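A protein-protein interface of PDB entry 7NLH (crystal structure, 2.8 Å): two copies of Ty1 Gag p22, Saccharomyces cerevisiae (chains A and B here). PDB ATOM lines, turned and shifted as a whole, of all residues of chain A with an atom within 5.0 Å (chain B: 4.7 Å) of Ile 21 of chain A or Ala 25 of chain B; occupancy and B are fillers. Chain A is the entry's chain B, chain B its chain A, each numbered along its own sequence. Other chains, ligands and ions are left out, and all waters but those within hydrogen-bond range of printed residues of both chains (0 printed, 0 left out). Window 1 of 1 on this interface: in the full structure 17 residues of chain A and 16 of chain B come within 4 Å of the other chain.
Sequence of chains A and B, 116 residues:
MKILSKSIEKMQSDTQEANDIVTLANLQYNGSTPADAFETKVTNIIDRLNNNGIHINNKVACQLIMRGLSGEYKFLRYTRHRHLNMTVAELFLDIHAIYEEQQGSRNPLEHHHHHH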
ATOM      1  N   GLU A  17     -15.103 -11.829   8.491  1.00  0.00           N
ATOM      2  CA  GLU A  17     -16.150 -11.923   9.537  1.00  0.00           C
ATOM      3  C   GLU A  17     -17.439 -11.312   8.988  1.00  0.00           C
ATOM      4  O   GLU A  17     -18.415 -12.055   8.834  1.00  0.00           O
ATOM      5  CB  GLU A  17     -15.722 -11.251  10.841  1.00  0.00           C
ATOM      6  CG  GLU A  17     -14.415 -11.780  11.405  1.00  0.00           C
ATOM      7  CD  GLU A  17     -13.210 -10.884  11.182  1.00  0.00           C
ATOM      8  OE1 GLU A  17     -13.306  -9.956  10.354  1.00  0.00           O
ATOM      9  OE2 GLU A  17     -12.177 -11.117  11.840  1.00  0.00           O
ATOM     10  N   ALA A  18     -17.427 -10.024   8.654  1.00  0.00           N
ATOM     11  CA  ALA A  18     -18.599  -9.276   8.146  1.00  0.00           C
ATOM     12  C   ALA A  18     -19.234 -10.003   6.953  1.00  0.00           C
ATOM     13  O   ALA A  18     -20.465  -9.909   6.824  1.00  0.00           O
ATOM     14  CB  ALA A  18     -18.206  -7.873   7.779  1.00  0.00           C
ATOM     15  N   ASN A  19     -18.449 -10.710   6.130  1.00  0.00           N
ATOM     16  CA  ASN A  19     -18.974 -11.491   4.975  1.00  0.00           C
ATOM     17  C   ASN A  19     -19.663 -12.770   5.468  1.00  0.00           C
ATOM     18  O   ASN A  19     -20.725 -13.126   4.909  1.00  0.00           O
ATOM     19  CB  ASN A  19     -17.885 -11.804   3.948  1.00  0.00           C
ATOM     20  CG  ASN A  19     -17.505 -10.580   3.148  1.00  0.00           C
ATOM     21  OD1 ASN A  19     -18.343  -9.711   2.921  1.00  0.00           O
ATOM     22  ND2 ASN A  19     -16.250 -10.494   2.728  1.00  0.00           N
ATOM     23  N   ASP A  20     -19.087 -13.442   6.469  1.00  0.00           N
ATOM     24  CA  ASP A  20     -19.675 -14.670   7.070  1.00  0.00           C
ATOM     25  C   ASP A  20     -20.977 -14.304   7.801  1.00  0.00           C
ATOM     26  O   ASP A  20     -21.989 -14.954   7.535  1.00  0.00           O
ATOM     27  CB  ASP A  20     -18.647 -15.389   7.943  1.00  0.00           C
ATOM     28  CG  ASP A  20     -17.464 -15.943   7.145  1.00  0.00           C
ATOM     29  OD1 ASP A  20     -17.675 -16.371   5.975  1.00  0.00           O
ATOM     30  OD2 ASP A  20     -16.339 -15.948   7.695  1.00  0.00           O
ATOM     31  N   ILE A  21     -20.965 -13.270   8.645  1.00  0.00           N
ATOM     32  CA  ILE A  21     -22.171 -12.766   9.373  1.00  0.00           C
ATOM     33  C   ILE A  21     -23.292 -12.465   8.371  1.00  0.00           C
ATOM     34  O   ILE A  21     -24.424 -12.838   8.658  1.00  0.00           O
ATOM     35  CB  ILE A  21     -21.833 -11.538  10.239  1.00  0.00           C
ATOM     36  CG1 ILE A  21     -21.064 -11.945  11.498  1.00  0.00           C
ATOM     37  CG2 ILE A  21     -23.082 -10.743  10.577  1.00  0.00           C
ATOM     38  CD1 ILE A  21     -20.387 -10.797  12.225  1.00  0.00           C
ATOM     39  N   VAL A  22     -23.006 -11.808   7.245  1.00  0.00           N
ATOM     40  CA  VAL A  22     -24.053 -11.424   6.246  1.00  0.00           C
ATOM     41  C   VAL A  22     -24.569 -12.686   5.539  1.00  0.00           C
ATOM     42  O   VAL A  22     -25.783 -12.753   5.289  1.00  0.00           O
ATOM     43  CB  VAL A  22     -23.553 -10.367   5.239  1.00  0.00           C
ATOM     44  CG1 VAL A  22     -24.452 -10.263   4.013  1.00  0.00           C
ATOM     45  CG2 VAL A  22     -23.405  -8.999   5.887  1.00  0.00           C
ATOM     46  N   THR A  23     -23.688 -13.631   5.197  1.00  0.00           N
ATOM     47  CA  THR A  23     -24.073 -14.914   4.554  1.00  0.00           C
ATOM     48  C   THR A  23     -25.011 -15.678   5.494  1.00  0.00           C
ATOM     49  O   THR A  23     -26.091 -16.124   5.041  1.00  0.00           O
ATOM     50  CB  THR A  23     -22.860 -15.791   4.238  1.00  0.00           C
ATOM     51  OG1 THR A  23     -22.029 -15.152   3.267  1.00  0.00           O
ATOM     52  CG2 THR A  23     -23.276 -17.153   3.724  1.00  0.00           C
ATOM     53  N   LEU A  24     -24.588 -15.811   6.756  1.00  0.00           N
ATOM     54  CA  LEU A  24     -25.258 -16.583   7.837  1.00  0.00           C
ATOM     55  C   LEU A  24     -26.646 -15.998   8.090  1.00  0.00           C
ATOM     56  O   LEU A  24     -27.586 -16.791   8.269  1.00  0.00           O
ATOM     57  CB  LEU A  24     -24.397 -16.506   9.103  1.00  0.00           C
ATOM     58  CG  LEU A  24     -24.822 -17.407  10.262  1.00  0.00           C
ATOM     59  CD1 LEU A  24     -24.547 -18.866   9.936  1.00  0.00           C
ATOM     60  CD2 LEU A  24     -24.113 -17.013  11.551  1.00  0.00           C
ATOM     61  N   ALA A  25     -26.762 -14.667   8.095  1.00  0.00           N
ATOM     62  CA  ALA A  25     -28.001 -13.923   8.419  1.00  0.00           C
ATOM     63  C   ALA A  25     -28.945 -13.860   7.210  1.00  0.00           C
ATOM     64  O   ALA A  25     -30.058 -13.321   7.379  1.00  0.00           O
ATOM     65  CB  ALA A  25     -27.660 -12.539   8.905  1.00  0.00           C
ATOM     66  N   ASN A  26     -28.542 -14.373   6.042  1.00  0.00           N
ATOM     67  CA  ASN A  26     -29.380 -14.335   4.813  1.00  0.00           C
ATOM     68  C   ASN A  26     -29.431 -15.720   4.143  1.00  0.00           C
ATOM     69  O   ASN A  26     -29.753 -15.772   2.940  1.00  0.00           O
ATOM     70  CB  ASN A  26     -28.888 -13.230   3.876  1.00  0.00           C
ATOM     71  CG  ASN A  26     -29.131 -11.842   4.437  1.00  0.00           C
ATOM     72  OD1 ASN A  26     -30.247 -11.324   4.364  1.00  0.00           O
ATOM     73  ND2 ASN A  26     -28.098 -11.228   5.000  1.00  0.00           N
ATOM     74  N   LEU A  49     -15.949 -17.882  11.992  1.00  0.00           N
ATOM     75  CA  LEU A  49     -16.388 -16.817  12.926  1.00  0.00           C
ATOM     76  C   LEU A  49     -15.806 -17.120  14.311  1.00  0.00           C
ATOM     77  O   LEU A  49     -15.387 -16.174  14.990  1.00  0.00           O
ATOM     78  CB  LEU A  49     -17.914 -16.724  12.942  1.00  0.00           C
ATOM     79  CG  LEU A  49     -18.547 -16.006  11.756  1.00  0.00           C
ATOM     80  CD1 LEU A  49     -20.045 -16.249  11.689  1.00  0.00           C
ATOM     81  CD2 LEU A  49     -18.295 -14.523  11.838  1.00  0.00           C
ATOM     82  N   ILE A  54     -15.551 -14.651  17.299  1.00  0.00           N
ATOM     83  CA  ILE A  54     -17.034 -14.463  17.281  1.00  0.00           C
ATOM     84  C   ILE A  54     -17.706 -15.832  17.440  1.00  0.00           C
ATOM     85  O   ILE A  54     -17.855 -16.534  16.426  1.00  0.00           O
ATOM     86  CB  ILE A  54     -17.514 -13.788  15.984  1.00  0.00           C
ATOM     87  CG1 ILE A  54     -16.867 -12.427  15.743  1.00  0.00           C
ATOM     88  CG2 ILE A  54     -19.033 -13.678  15.962  1.00  0.00           C
ATOM     89  CD1 ILE A  54     -17.278 -11.799  14.416  1.00  0.00           C
ATOM     90  N   ILE B  21     -28.207 -10.099  15.173  1.00  0.00           N
ATOM     91  CA  ILE B  21     -27.295 -10.514  14.064  1.00  0.00           C
ATOM     92  C   ILE B  21     -27.944 -10.203  12.707  1.00  0.00           C
ATOM     93  O   ILE B  21     -27.251  -9.672  11.840  1.00  0.00           O
ATOM     94  CB  ILE B  21     -26.907 -12.000  14.178  1.00  0.00           C
ATOM     95  CG1 ILE B  21     -25.922 -12.235  15.320  1.00  0.00           C
ATOM     96  CG2 ILE B  21     -26.374 -12.519  12.851  1.00  0.00           C
ATOM     97  CD1 ILE B  21     -25.751 -13.689  15.687  1.00  0.00           C
ATOM     98  N   VAL B  22     -29.220 -10.538  12.511  1.00  0.00           N
ATOM     99  CA  VAL B  22     -29.910 -10.355  11.198  1.00  0.00           C
ATOM    100  C   VAL B  22     -30.148  -8.858  10.956  1.00  0.00           C
ATOM    101  O   VAL B  22     -30.013  -8.435   9.803  1.00  0.00           O
ATOM    102  CB  VAL B  22     -31.211 -11.176  11.106  1.00  0.00           C
ATOM    103  CG1 VAL B  22     -32.112 -10.711   9.971  1.00  0.00           C
ATOM    104  CG2 VAL B  22     -30.912 -12.660  10.956  1.00  0.00           C
ATOM    105  N   THR B  23     -30.521  -8.091  11.985  1.00  0.00           N
ATOM    106  CA  THR B  23     -30.717  -6.618  11.892  1.00  0.00           C
ATOM    107  C   THR B  23     -29.400  -5.975  11.458  1.00  0.00           C
ATOM    108  O   THR B  23     -29.417  -5.184  10.494  1.00  0.00           O
ATOM    109  CB  THR B  23     -31.144  -5.993  13.226  1.00  0.00           C
ATOM    110  OG1 THR B  23     -32.442  -6.477  13.574  1.00  0.00           O
ATOM    111  CG2 THR B  23     -31.158  -4.479  13.179  1.00  0.00           C
ATOM    112  N   LEU B  24     -28.321  -6.326  12.168  1.00  0.00           N
ATOM    113  CA  LEU B  24     -26.951  -5.770  12.023  1.00  0.00           C
ATOM    114  C   LEU B  24     -26.432  -6.056  10.614  1.00  0.00           C
ATOM    115  O   LEU B  24     -25.832  -5.148  10.028  1.00  0.00           O
ATOM    116  CB  LEU B  24     -26.051  -6.408  13.087  1.00  0.00           C
ATOM    117  CG  LEU B  24     -24.652  -5.813  13.225  1.00  0.00           C
ATOM    118  CD1 LEU B  24     -24.717  -4.435  13.858  1.00  0.00           C
ATOM    119  CD2 LEU B  24     -23.753  -6.732  14.035  1.00  0.00           C
ATOM    120  N   ALA B  25     -26.682  -7.264  10.101  1.00  0.00           N
ATOM    121  CA  ALA B  25     -26.188  -7.759   8.795  1.00  0.00           C
ATOM    122  C   ALA B  25     -27.043  -7.236   7.632  1.00  0.00           C
ATOM    123  O   ALA B  25     -26.680  -7.517   6.475  1.00  0.00           O
ATOM    124  CB  ALA B  25     -26.152  -9.266   8.795  1.00  0.00           C
ATOM    125  N   ASN B  26     -28.133  -6.515   7.904  1.00  0.00           N
ATOM    126  CA  ASN B  26     -29.045  -5.999   6.847  1.00  0.00           C
ATOM    127  C   ASN B  26     -29.362  -4.516   7.090  1.00  0.00           C
ATOM    128  O   ASN B  26     -30.390  -4.045   6.564  1.00  0.00           O
ATOM    129  CB  ASN B  26     -30.303  -6.866   6.755  1.00  0.00           C
ATOM    130  CG  ASN B  26     -30.011  -8.256   6.229  1.00  0.00           C
ATOM    131  OD1 ASN B  26     -29.866  -8.454   5.025  1.00  0.00           O
ATOM    132  ND2 ASN B  26     -29.926  -9.229   7.122  1.00  0.00           N
ATOM    133  N   LEU B  27     -28.503  -3.796   7.821  1.00  0.00           N
ATOM    134  CA  LEU B  27     -28.661  -2.339   8.077  1.00  0.00           C
ATOM    135  C   LEU B  27     -28.766  -1.605   6.737  1.00  0.00           C
ATOM    136  O   LEU B  27     -28.073  -2.009   5.786  1.00  0.00           O
ATOM    137  CB  LEU B  27     -27.475  -1.818   8.896  1.00  0.00           C
ATOM    138  CG  LEU B  27     -27.516  -2.141  10.389  1.00  0.00           C
ATOM    139  CD1 LEU B  27     -26.148  -1.949  11.029  1.00  0.00           C
ATOM    140  CD2 LEU B  27     -28.559  -1.293  11.109  1.00  0.00           C
ATOM    141  N   ILE B  56     -18.610  -8.508  18.699  1.00  0.00           N
ATOM    142  CA  ILE B  56     -18.463  -7.771  17.413  1.00  0.00           C
ATOM    143  C   ILE B  56     -17.585  -6.554  17.705  1.00  0.00           C
ATOM    144  O   ILE B  56     -18.116  -5.518  18.145  1.00  0.00           O
ATOM    145  CB  ILE B  56     -19.826  -7.359  16.820  1.00  0.00           C
ATOM    146  CG1 ILE B  56     -20.815  -8.521  16.749  1.00  0.00           C
ATOM    147  CG2 ILE B  56     -19.636  -6.714  15.462  1.00  0.00           C
ATOM    148  CD1 ILE B  56     -20.289  -9.734  16.038  1.00  0.00           C
ATOM    149  N   VAL B  60     -15.220  -5.034  12.665  1.00  0.00           N
ATOM    150  CA  VAL B  60     -16.318  -5.796  12.009  1.00  0.00           C
ATOM    151  C   VAL B  60     -17.631  -5.009  12.147  1.00  0.00           C
ATOM    152  O   VAL B  60     -18.371  -4.954  11.154  1.00  0.00           O
ATOM    153  CB  VAL B  60     -16.399  -7.251  12.503  1.00  0.00           C
ATOM    154  CG1 VAL B  60     -16.441  -7.392  14.013  1.00  0.00           C
ATOM    155  CG2 VAL B  60     -17.569  -7.977  11.859  1.00  0.00           C
ATOM    156  N   LEU B  64     -19.902  -3.525   8.913  1.00  0.00           N
ATOM    157  CA  LEU B  64     -21.336  -3.891   8.754  1.00  0.00           C
ATOM    158  C   LEU B  64     -22.203  -2.633   8.709  1.00  0.00           C
ATOM    159  O   LEU B  64     -23.229  -2.673   8.012  1.00  0.00           O
ATOM    160  CB  LEU B  64     -21.760  -4.819   9.896  1.00  0.00           C
ATOM    161  CG  LEU B  64     -21.196  -6.232   9.813  1.00  0.00           C
ATOM    162  CD1 LEU B  64     -21.408  -6.974  11.118  1.00  0.00           C
ATOM    163  CD2 LEU B  64     -21.813  -6.988   8.647  1.00  0.00           C
ATOM    164  N   ARG B  67     -21.366  -0.974   5.062  1.00  0.00           N
ATOM    165  CA  ARG B  67     -22.202  -1.748   4.111  1.00  0.00           C
ATOM    166  C   ARG B  67     -23.622  -1.203   4.263  1.00  0.00           C
ATOM    167  O   ARG B  67     -23.983  -0.859   5.407  1.00  0.00           O
ATOM    168  CB  ARG B  67     -22.109  -3.245   4.423  1.00  0.00           C
ATOM    169  CG  ARG B  67     -22.721  -4.145   3.360  1.00  0.00           C
ATOM    170  CD  ARG B  67     -22.607  -5.613   3.733  1.00  0.00           C
ATOM    171  NE  ARG B  67     -23.752  -6.404   3.307  1.00  0.00           N
ATOM    172  CZ  ARG B  67     -24.976  -6.308   3.824  1.00  0.00           C
ATOM    173  NH1 ARG B  67     -25.242  -5.437   4.788  1.00  0.00           N
ATOM    174  NH2 ARG B  67     -25.939  -7.093   3.372  1.00  0.00           N
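Printed residues of chain A that touch a printed residue of chain B: Glu 17, Ala 18, Ile 21, Val 22, Ala 25, Asn 26 and Ile 54. Hydrophobic or aromatic side chains of chain A that line the printed part of chain B: Ala 18, Ile 21, Val 22, Ala 25 and Ile 54. Hydrophobic or aromatic side chains of chain B within 4 Å of the printed part of chain A: Val 22, Ala 25, Ile 56, Val 60 and Leu 64. Among the printed residues, 12 pairs touch across the chains.
The side-chain amide nitrogen of Asn 26 of chain B is in hydrogen-bond range of the backbone carbonyl oxygen of Val 22 of chain B, at 2.8 Å. The backbone carbonyl oxygen (O) of Ala 25 of chain B lies within hydrogen-bond range of the guanidinium group (NH1) of Arg 67 of chain B (3.0 Å). The side-chain amide nitrogen (ND2) of Asn 26 of chain A is in hydrogen-bond range of the backbone carbonyl oxygen (O) of Val 22 of chain A (2.8 Å). The backbone carbonyl oxygen (O) of Leu 49 of chain A lies within hydrogen-bond range of the backbone NH (N) of Ile 54 of chain A (2.8 Å).
Among the printed residues, pairs that only touch across the chains: Glu 17 of chain A with Val 60 of chain B (3.9 Å), Ala 18 of chain A with Val 60 of chain B (3.8 Å), Ala 18 of chain A with Leu 64 of chain B (3.7 Å), Ile 21 of chain A with Ala 25 of chain B (3.8 Å), Ile 21 of chain A with Ile 56 of chain B (3.96 Å), Val 22 of chain A with Ala 25 of chain B (3.6 Å), Val 22 of chain A with Leu 64 of chain B (3.8 Å), Val 22 of chain A with Arg 67 of chain B (3.6 Å), Ala 25 of chain A with Val 22 of chain B (3.7 Å), Ala 25 of chain A with Ala 25 of chain B (3.6 Å) and Ile 54 of chain A with Ile 56 of chain B (3.995 Å).
Ile 21 of chain A touches Ala 25 of chain B, but with the chains exchanged Ala 25 of chain A does not touch Ile 21 of chain B (4.1 Å). Val 22 of chain A touches Ala 25 of chain B, and with the chains exchanged Ala 25 of chain A touches Val 22 of chain B. Ala 25 of chain A touches its own counterpart, Ala 25 of chain B. Asn 26 of chain B touches its own counterpart, Asn 26 of chain A. Positions printed for both chains: 21, 22, 23, 24, 25 and 26. Of the 12 pairs that touch across the chains among the printed residues, 4 have their exchanged pair printed and touching as well.
Printed residues of chain B within 4 Å of Ile 21 of chain A: Ala 25 (3.8 Å) and Ile 56 (3.96 Å). Ala 25 of chain B touches three residues of chain A. Of the printed residues of chain B, Ile 54 of chain A touches Ile 56. Of the printed residues of chain A, Asn 26 of chain B touches Asn 26 (3.0 Å). Leu 49 of chain A touches none of the printed residues of chain B. The nearest printed residue of chain B that does not touch Ile 21 of chain A is Val 60 of chain B (4.003 Å). The nearest residue of chain A that does not touch Ala 25 of chain B is Asn 26 of chain A (4.2 Å).
The side-chain amide oxygen (OD1) of Asn 26 of chain B lies close to the side-chain amide oxygen (OD1) of Asn 26 of chain A, at 3.0 Å.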
